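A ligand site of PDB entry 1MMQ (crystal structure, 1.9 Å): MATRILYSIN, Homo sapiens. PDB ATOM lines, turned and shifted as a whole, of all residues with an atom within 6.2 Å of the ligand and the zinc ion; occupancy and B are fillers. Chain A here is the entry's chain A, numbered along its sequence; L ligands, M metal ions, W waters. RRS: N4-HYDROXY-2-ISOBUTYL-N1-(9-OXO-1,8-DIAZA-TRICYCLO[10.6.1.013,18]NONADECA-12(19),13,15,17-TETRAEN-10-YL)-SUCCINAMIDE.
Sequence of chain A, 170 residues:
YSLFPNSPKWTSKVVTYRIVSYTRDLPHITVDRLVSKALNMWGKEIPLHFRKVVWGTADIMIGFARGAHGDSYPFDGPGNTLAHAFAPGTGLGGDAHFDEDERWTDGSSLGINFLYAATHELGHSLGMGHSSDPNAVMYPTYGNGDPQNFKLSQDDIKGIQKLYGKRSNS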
ATOM      1  N   ASP A  76     -10.487 -23.485 -14.036  1.00  0.00           N
ATOM      2  CA  ASP A  76     -10.139 -22.349 -14.891  1.00  0.00           C
ATOM      3  C   ASP A  76      -8.698 -21.902 -14.909  1.00  0.00           C
ATOM      4  O   ASP A  76      -8.432 -20.778 -15.319  1.00  0.00           O
ATOM      5  CB  ASP A  76     -11.010 -21.250 -14.378  1.00  0.00           C
ATOM      6  CG  ASP A  76     -10.769 -21.022 -12.853  1.00  0.00           C
ATOM      7  OD1 ASP A  76      -9.798 -21.483 -12.181  1.00  0.00           O
ATOM      8  OD2 ASP A  76     -11.626 -20.344 -12.328  1.00  0.00           O
ATOM      9  N   GLY A  79      -5.670 -18.764 -10.356  1.00  0.00           N
ATOM     10  CA  GLY A  79      -6.620 -17.737  -9.949  1.00  0.00           C
ATOM     11  C   GLY A  79      -8.061 -18.147 -10.186  1.00  0.00           C
ATOM     12  O   GLY A  79      -8.402 -19.338 -10.464  1.00  0.00           O
ATOM     13  N   ASN A  80      -8.890 -17.122 -10.018  1.00  0.00           N
ATOM     14  CA  ASN A  80     -10.359 -17.199 -10.143  1.00  0.00           C
ATOM     15  C   ASN A  80     -10.832 -18.307  -9.213  1.00  0.00           C
ATOM     16  O   ASN A  80     -10.588 -18.180  -8.024  1.00  0.00           O
ATOM     17  CB  ASN A  80     -10.701 -17.438 -11.637  1.00  0.00           C
ATOM     18  CG  ASN A  80     -10.416 -16.199 -12.474  1.00  0.00           C
ATOM     19  OD1 ASN A  80     -10.503 -16.207 -13.704  1.00  0.00           O
ATOM     20  ND2 ASN A  80     -10.106 -15.043 -11.912  1.00  0.00           N
ATOM     21  N   THR A  81     -11.500 -19.366  -9.643  1.00  0.00           N
ATOM     22  CA  THR A  81     -11.918 -20.442  -8.754  1.00  0.00           C
ATOM     23  C   THR A  81     -10.681 -21.255  -8.390  1.00  0.00           C
ATOM     24  O   THR A  81      -9.844 -21.655  -9.248  1.00  0.00           O
ATOM     25  CB  THR A  81     -12.960 -21.306  -9.471  1.00  0.00           C
ATOM     26  OG1 THR A  81     -14.059 -20.449  -9.851  1.00  0.00           O
ATOM     27  CG2 THR A  81     -13.441 -22.466  -8.608  1.00  0.00           C
ATOM     28  N   LEU A  82     -10.558 -21.401  -7.072  1.00  0.00           N
ATOM     29  CA  LEU A  82      -9.476 -22.139  -6.394  1.00  0.00           C
ATOM     30  C   LEU A  82      -9.749 -23.633  -6.135  1.00  0.00           C
ATOM     31  O   LEU A  82      -8.857 -24.477  -6.200  1.00  0.00           O
ATOM     32  CB  LEU A  82      -9.214 -21.400  -5.074  1.00  0.00           C
ATOM     33  CG  LEU A  82      -8.203 -20.249  -5.012  1.00  0.00           C
ATOM     34  CD1 LEU A  82      -8.036 -19.509  -6.338  1.00  0.00           C
ATOM     35  CD2 LEU A  82      -8.647 -19.419  -3.801  1.00  0.00           C
ATOM     36  N   ALA A  83     -10.991 -23.958  -5.813  1.00  0.00           N
ATOM     37  CA  ALA A  83     -11.419 -25.316  -5.479  1.00  0.00           C
ATOM     38  C   ALA A  83     -12.951 -25.325  -5.378  1.00  0.00           C
ATOM     39  O   ALA A  83     -13.579 -24.249  -5.421  1.00  0.00           O
ATOM     40  CB  ALA A  83     -10.785 -25.675  -4.103  1.00  0.00           C
ATOM     41  N   HIS A  84     -13.579 -26.499  -5.298  1.00  0.00           N
ATOM     42  CA  HIS A  84     -15.032 -26.586  -5.154  1.00  0.00           C
ATOM     43  C   HIS A  84     -15.353 -27.928  -4.512  1.00  0.00           C
ATOM     44  O   HIS A  84     -14.546 -28.857  -4.562  1.00  0.00           O
ATOM     45  CB  HIS A  84     -15.802 -26.456  -6.541  1.00  0.00           C
ATOM     46  CG  HIS A  84     -15.407 -27.403  -7.672  1.00  0.00           C
ATOM     47  ND1 HIS A  84     -15.216 -26.989  -8.898  1.00  0.00           N
ATOM     48  CD2 HIS A  84     -15.159 -28.758  -7.616  1.00  0.00           C
ATOM     49  CE1 HIS A  84     -14.845 -28.011  -9.616  1.00  0.00           C
ATOM     50  NE2 HIS A  84     -14.816 -29.056  -8.834  1.00  0.00           N
ATOM     51  N   ALA A  85     -16.544 -28.048  -3.951  1.00  0.00           N
ATOM     52  CA  ALA A  85     -16.954 -29.283  -3.273  1.00  0.00           C
ATOM     53  C   ALA A  85     -18.461 -29.478  -3.426  1.00  0.00           C
ATOM     54  O   ALA A  85     -19.178 -28.562  -3.856  1.00  0.00           O
ATOM     55  CB  ALA A  85     -16.572 -29.224  -1.760  1.00  0.00           C
ATOM     56  N   ILE A 112      -1.663 -20.090  -2.261  1.00  0.00           N
ATOM     57  CA  ILE A 112      -2.971 -20.262  -1.617  1.00  0.00           C
ATOM     58  C   ILE A 112      -2.772 -21.277  -0.493  1.00  0.00           C
ATOM     59  O   ILE A 112      -2.218 -22.376  -0.694  1.00  0.00           O
ATOM     60  CB  ILE A 112      -3.995 -20.790  -2.636  1.00  0.00           C
ATOM     61  CG1 ILE A 112      -3.956 -19.941  -3.949  1.00  0.00           C
ATOM     62  CG2 ILE A 112      -5.381 -20.778  -1.946  1.00  0.00           C
ATOM     63  CD1 ILE A 112      -4.451 -18.486  -3.818  1.00  0.00           C
ATOM     64  N   TYR A 116      -6.581 -23.499   4.859  1.00  0.00           N
ATOM     65  CA  TYR A 116      -7.743 -22.624   4.807  1.00  0.00           C
ATOM     66  C   TYR A 116      -8.717 -23.129   3.718  1.00  0.00           C
ATOM     67  O   TYR A 116      -9.906 -23.312   3.994  1.00  0.00           O
ATOM     68  CB  TYR A 116      -7.297 -21.136   4.504  1.00  0.00           C
ATOM     69  CG  TYR A 116      -8.489 -20.243   4.604  1.00  0.00           C
ATOM     70  CD1 TYR A 116      -9.331 -20.045   3.480  1.00  0.00           C
ATOM     71  CD2 TYR A 116      -8.852 -19.695   5.855  1.00  0.00           C
ATOM     72  CE1 TYR A 116     -10.507 -19.314   3.597  1.00  0.00           C
ATOM     73  CE2 TYR A 116     -10.043 -18.965   5.974  1.00  0.00           C
ATOM     74  CZ  TYR A 116     -10.862 -18.777   4.847  1.00  0.00           C
ATOM     75  OH  TYR A 116     -12.040 -18.038   4.958  1.00  0.00           O
ATOM     76  N   ALA A 117      -8.233 -23.346   2.482  1.00  0.00           N
ATOM     77  CA  ALA A 117      -9.076 -23.812   1.373  1.00  0.00           C
ATOM     78  C   ALA A 117      -9.743 -25.137   1.720  1.00  0.00           C
ATOM     79  O   ALA A 117     -10.935 -25.291   1.496  1.00  0.00           O
ATOM     80  CB  ALA A 117      -8.258 -24.011   0.080  1.00  0.00           C
ATOM     81  N   ALA A 118      -9.014 -26.097   2.274  1.00  0.00           N
ATOM     82  CA  ALA A 118      -9.576 -27.404   2.648  1.00  0.00           C
ATOM     83  C   ALA A 118     -10.634 -27.224   3.734  1.00  0.00           C
ATOM     84  O   ALA A 118     -11.677 -27.873   3.671  1.00  0.00           O
ATOM     85  CB  ALA A 118      -8.503 -28.343   3.195  1.00  0.00           C
ATOM     86  N   HIS A 120     -12.596 -24.729   4.173  1.00  0.00           N
ATOM     87  CA  HIS A 120     -13.778 -24.186   3.454  1.00  0.00           C
ATOM     88  C   HIS A 120     -14.465 -25.322   2.626  1.00  0.00           C
ATOM     89  O   HIS A 120     -15.663 -25.584   2.748  1.00  0.00           O
ATOM     90  CB  HIS A 120     -13.295 -23.003   2.536  1.00  0.00           C
ATOM     91  CG  HIS A 120     -14.430 -22.410   1.700  1.00  0.00           C
ATOM     92  ND1 HIS A 120     -15.099 -21.310   1.987  1.00  0.00           N
ATOM     93  CD2 HIS A 120     -14.967 -22.946   0.544  1.00  0.00           C
ATOM     94  CE1 HIS A 120     -16.016 -21.128   1.066  1.00  0.00           C
ATOM     95  NE2 HIS A 120     -15.917 -22.120   0.215  1.00  0.00           N
ATOM     96  N   GLU A 121     -13.718 -25.996   1.751  1.00  0.00           N
ATOM     97  CA  GLU A 121     -14.305 -27.066   0.948  1.00  0.00           C
ATOM     98  C   GLU A 121     -14.906 -28.184   1.767  1.00  0.00           C
ATOM     99  O   GLU A 121     -16.012 -28.642   1.453  1.00  0.00           O
ATOM    100  CB  GLU A 121     -13.219 -27.632  -0.001  1.00  0.00           C
ATOM    101  CG  GLU A 121     -12.640 -26.647  -1.073  1.00  0.00           C
ATOM    102  CD  GLU A 121     -13.632 -25.607  -1.646  1.00  0.00           C
ATOM    103  OE1 GLU A 121     -14.788 -25.932  -1.905  1.00  0.00           O
ATOM    104  OE2 GLU A 121     -13.260 -24.459  -1.872  1.00  0.00           O
ATOM    105  N   HIS A 124     -18.367 -27.580   2.958  1.00  0.00           N
ATOM    106  CA  HIS A 124     -19.393 -27.939   1.961  1.00  0.00           C
ATOM    107  C   HIS A 124     -19.615 -29.449   1.982  1.00  0.00           C
ATOM    108  O   HIS A 124     -20.762 -29.894   1.916  1.00  0.00           O
ATOM    109  CB  HIS A 124     -19.000 -27.618   0.503  1.00  0.00           C
ATOM    110  CG  HIS A 124     -19.056 -26.140   0.217  1.00  0.00           C
ATOM    111  ND1 HIS A 124     -20.071 -25.333   0.453  1.00  0.00           N
ATOM    112  CD2 HIS A 124     -18.041 -25.436  -0.346  1.00  0.00           C
ATOM    113  CE1 HIS A 124     -19.734 -24.136   0.067  1.00  0.00           C
ATOM    114  NE2 HIS A 124     -18.530 -24.221  -0.398  1.00  0.00           N
ATOM    115  N   HIS A 130     -22.592 -21.153   1.700  1.00  0.00           N
ATOM    116  CA  HIS A 130     -21.764 -19.949   1.888  1.00  0.00           C
ATOM    117  C   HIS A 130     -22.409 -18.996   2.848  1.00  0.00           C
ATOM    118  O   HIS A 130     -23.630 -18.868   2.937  1.00  0.00           O
ATOM    119  CB  HIS A 130     -21.577 -19.205   0.594  1.00  0.00           C
ATOM    120  CG  HIS A 130     -20.629 -19.938  -0.315  1.00  0.00           C
ATOM    121  ND1 HIS A 130     -20.668 -19.845  -1.629  1.00  0.00           N
ATOM    122  CD2 HIS A 130     -19.503 -20.615   0.092  1.00  0.00           C
ATOM    123  CE1 HIS A 130     -19.590 -20.440  -2.058  1.00  0.00           C
ATOM    124  NE2 HIS A 130     -18.912 -20.880  -1.021  1.00  0.00           N
ATOM    125  N   VAL A 137     -15.309 -18.693   7.710  1.00  0.00           N
ATOM    126  CA  VAL A 137     -14.502 -19.523   6.814  1.00  0.00           C
ATOM    127  C   VAL A 137     -15.365 -19.839   5.590  1.00  0.00           C
ATOM    128  O   VAL A 137     -14.848 -19.939   4.465  1.00  0.00           O
ATOM    129  CB  VAL A 137     -14.087 -20.846   7.502  1.00  0.00           C
ATOM    130  CG1 VAL A 137     -13.320 -21.748   6.523  1.00  0.00           C
ATOM    131  CG2 VAL A 137     -13.209 -20.484   8.715  1.00  0.00           C
ATOM    132  N   MET A 138     -16.696 -20.008   5.774  1.00  0.00           N
ATOM    133  CA  MET A 138     -17.568 -20.310   4.622  1.00  0.00           C
ATOM    134  C   MET A 138     -17.881 -19.116   3.733  1.00  0.00           C
ATOM    135  O   MET A 138     -18.714 -19.222   2.828  1.00  0.00           O
ATOM    136  CB  MET A 138     -18.888 -20.951   5.121  1.00  0.00           C
ATOM    137  CG  MET A 138     -18.618 -22.334   5.738  1.00  0.00           C
ATOM    138  SD  MET A 138     -17.519 -23.449   4.785  1.00  0.00           S
ATOM    139  CE  MET A 138     -18.369 -23.599   3.204  1.00  0.00           C
ATOM    140  N   TYR A 139     -17.232 -17.959   3.944  1.00  0.00           N
ATOM    141  CA  TYR A 139     -17.484 -16.801   3.058  1.00  0.00           C
ATOM    142  C   TYR A 139     -16.983 -17.182   1.650  1.00  0.00           C
ATOM    143  O   TYR A 139     -16.030 -17.962   1.518  1.00  0.00           O
ATOM    144  CB  TYR A 139     -16.715 -15.558   3.565  1.00  0.00           C
ATOM    145  CG  TYR A 139     -17.227 -14.348   2.925  1.00  0.00           C
ATOM    146  CD1 TYR A 139     -18.519 -13.874   3.240  1.00  0.00           C
ATOM    147  CD2 TYR A 139     -16.412 -13.666   1.988  1.00  0.00           C
ATOM    148  CE1 TYR A 139     -19.010 -12.711   2.615  1.00  0.00           C
ATOM    149  CE2 TYR A 139     -16.903 -12.519   1.358  1.00  0.00           C
ATOM    150  CZ  TYR A 139     -18.194 -12.045   1.673  1.00  0.00           C
ATOM    151  OH  TYR A 139     -18.656 -10.905   1.044  1.00  0.00           O
ATOM    152  N   PRO A 140     -17.601 -16.714   0.565  1.00  0.00           N
ATOM    153  CA  PRO A 140     -17.195 -17.191  -0.774  1.00  0.00           C
ATOM    154  C   PRO A 140     -15.844 -16.755  -1.351  1.00  0.00           C
ATOM    155  O   PRO A 140     -15.352 -17.403  -2.268  1.00  0.00           O
ATOM    156  CB  PRO A 140     -18.389 -16.823  -1.670  1.00  0.00           C
ATOM    157  CG  PRO A 140     -19.047 -15.666  -0.924  1.00  0.00           C
ATOM    158  CD  PRO A 140     -18.922 -16.070   0.525  1.00  0.00           C
ATOM    159  N   THR A 141     -15.228 -15.682  -0.888  1.00  0.00           N
ATOM    160  CA  THR A 141     -13.921 -15.252  -1.427  1.00  0.00           C
ATOM    161  C   THR A 141     -12.794 -15.595  -0.461  1.00  0.00           C
ATOM    162  O   THR A 141     -12.962 -15.658   0.767  1.00  0.00           O
ATOM    163  CB  THR A 141     -13.980 -13.720  -1.674  1.00  0.00           C
ATOM    164  OG1 THR A 141     -14.449 -13.076  -0.485  1.00  0.00           O
ATOM    165  CG2 THR A 141     -14.913 -13.367  -2.836  1.00  0.00           C
ATOM    166  N   TYR A 142     -11.592 -15.752  -1.004  1.00  0.00           N
ATOM    167  CA  TYR A 142     -10.401 -16.095  -0.226  1.00  0.00           C
ATOM    168  C   TYR A 142      -9.621 -14.847   0.186  1.00  0.00           C
ATOM    169  O   TYR A 142      -9.612 -13.888  -0.586  1.00  0.00           O
ATOM    170  CB  TYR A 142      -9.501 -16.983  -1.107  1.00  0.00           C
ATOM    171  CG  TYR A 142      -8.205 -17.302  -0.496  1.00  0.00           C
ATOM    172  CD1 TYR A 142      -8.121 -18.418   0.361  1.00  0.00           C
ATOM    173  CD2 TYR A 142      -7.080 -16.519  -0.783  1.00  0.00           C
ATOM    174  CE1 TYR A 142      -6.890 -18.745   0.931  1.00  0.00           C
ATOM    175  CE2 TYR A 142      -5.848 -16.837  -0.202  1.00  0.00           C
ATOM    176  CZ  TYR A 142      -5.764 -17.953   0.655  1.00  0.00           C
ATOM    177  OH  TYR A 142      -4.547 -18.280   1.228  1.00  0.00           O
ATOM    178  N   GLY A 143      -8.975 -14.838   1.353  1.00  0.00           N
ATOM    179  CA  GLY A 143      -8.126 -13.706   1.775  1.00  0.00           C
ATOM    180  C   GLY A 143      -8.663 -12.587   2.654  1.00  0.00           C
ATOM    181  O   GLY A 143      -7.924 -11.657   2.942  1.00  0.00           O
HETATM  182  C1  RRS L   1     -15.694 -21.933  -3.457  1.00  0.00           C
HETATM  183  O2  RRS L   1     -16.397 -21.154  -2.760  1.00  0.00           O
HETATM  184  N1  RRS L   1     -15.511 -23.230  -3.491  1.00  0.00           N
HETATM  185  O1  RRS L   1     -16.277 -23.937  -2.568  1.00  0.00           O
HETATM  186  C2  RRS L   1     -14.822 -21.071  -4.325  1.00  0.00           C
HETATM  187  C3  RRS L   1     -13.807 -20.291  -3.440  1.00  0.00           C
HETATM  188  C4  RRS L   1     -13.051 -19.431  -4.427  1.00  0.00           C
HETATM  189  O3  RRS L   1     -12.221 -19.911  -5.203  1.00  0.00           O
HETATM  190  N2  RRS L   1     -13.348 -18.143  -4.389  1.00  0.00           N
HETATM  191  C5  RRS L   1     -12.754 -17.201  -5.321  1.00  0.00           C
HETATM  192  C6  RRS L   1     -11.501 -16.483  -4.841  1.00  0.00           C
HETATM  193  O4  RRS L   1     -11.481 -15.892  -3.763  1.00  0.00           O
HETATM  194  N3  RRS L   1     -10.470 -16.452  -5.674  1.00  0.00           N
HETATM  195  C7  RRS L   1      -9.212 -15.752  -5.371  1.00  0.00           C
HETATM  196  C8  RRS L   1      -8.511 -15.401  -6.711  1.00  0.00           C
HETATM  197  C9  RRS L   1      -9.371 -14.534  -7.653  1.00  0.00           C
HETATM  198  C10 RRS L   1      -9.504 -13.052  -7.237  1.00  0.00           C
HETATM  199  C11 RRS L   1     -10.391 -12.204  -8.179  1.00  0.00           C
HETATM  200  C12 RRS L   1     -11.886 -12.036  -7.805  1.00  0.00           C
HETATM  201  N4  RRS L   1     -12.594 -13.322  -7.663  1.00  0.00           N
HETATM  202  C13 RRS L   1     -12.852 -21.186  -2.614  1.00  0.00           C
HETATM  203  C14 RRS L   1     -12.015 -20.411  -1.566  1.00  0.00           C
HETATM  204  C15 RRS L   1     -12.895 -19.649  -0.554  1.00  0.00           C
HETATM  205  C16 RRS L   1     -11.168 -21.436  -0.797  1.00  0.00           C
HETATM  206  C17 RRS L   1     -13.898 -16.204  -5.687  1.00  0.00           C
HETATM  207  C18 RRS L   1     -13.476 -15.210  -6.702  1.00  0.00           C
HETATM  208  C19 RRS L   1     -12.885 -13.947  -6.486  1.00  0.00           C
HETATM  209  C20 RRS L   1     -13.542 -15.345  -8.106  1.00  0.00           C
HETATM  210  C21 RRS L   1     -12.994 -14.153  -8.677  1.00  0.00           C
HETATM  211  C22 RRS L   1     -14.028 -16.369  -8.929  1.00  0.00           C
HETATM  212  C23 RRS L   1     -12.935 -14.006 -10.065  1.00  0.00           C
HETATM  213  C24 RRS L   1     -13.971 -16.214 -10.323  1.00  0.00           C
HETATM  214  C25 RRS L   1     -13.432 -15.047 -10.874  1.00  0.00           C
HETATM  215 ZN    ZN M   1     -17.369 -22.469  -1.351  1.00  0.00          ZN
HETATM  216  O   HOH W   1     -18.035 -25.390  -4.006  1.00  0.00           O
HETATM  217  O   HOH W   2     -17.094 -18.937  -4.186  1.00  0.00           O
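A ring nitrogen (ND1) of His 120 sits at hydrogen-bond distance from the backbone carbonyl oxygen (O) of Val 137 (2.8 Å). The side-chain carboxylate (OE1) of Glu 121 lies within hydrogen-bond range of the backbone NH (N) of Ala 85 (3.4 Å).
The nearest printed residue that does not touch the zinc ion is Glu 121 (4.4 Å).
Thr 81 touches the ligand. His 84 touches the ligand (CA to N1, 3.8 Å). Ala 117 touches the ligand (CA to C16, 3.8 Å). Thr 141 touches the ligand. Hydrophobic or aromatic side chains within 4 Å of the ligand: Leu 82, Ala 117, His 120, His 124, His 130 and Tyr 142. Within 4 Å of the ligand: Asn 80, Thr 81, Leu 82, Ala 83, His 84, Ala 117, His 120, Glu 121, His 124, His 130, Pro 140, Thr 141 and Tyr 142.
The side-chain carboxylate (OE2) of Glu 121 is in hydrogen-bond range of a nitrogen (N1) of the ligand (3.0 Å). The backbone NH (N) of Tyr 142 is in hydrogen-bond range of an oxygen (O4) of the ligand, at 2.8 Å. An oxygen (O3) of the ligand lies within hydrogen-bond range of the backbone NH of Leu 82 (2.9 Å). A nitrogen (N1) of the ligand is in hydrogen-bond range of the backbone carbonyl oxygen (O) of Ala 83, at 2.9 Å. O of Asn 80 sits at hydrogen-bond distance from N3 of the ligand (2.9 Å). A nitrogen (N2) of the ligand sits at hydrogen-bond distance from the backbone carbonyl oxygen (O) of Pro 140 (3.0 Å).
Water W1 lies within hydrogen-bond range of the backbone NH of Ala 85 (3.0 Å) and a nitrogen (N1) of the ligand (3.4 Å).
The zinc ion is bound by an oxygen (O2) of the ligand (2.2 Å), a ring nitrogen (NE2) of His 120 (2.2 Å), an oxygen (O1) of the ligand (2.2 Å), a ring nitrogen (NE2) of His 130 (2.2 Å) and a ring nitrogen (NE2) of His 124 (2.3 Å).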
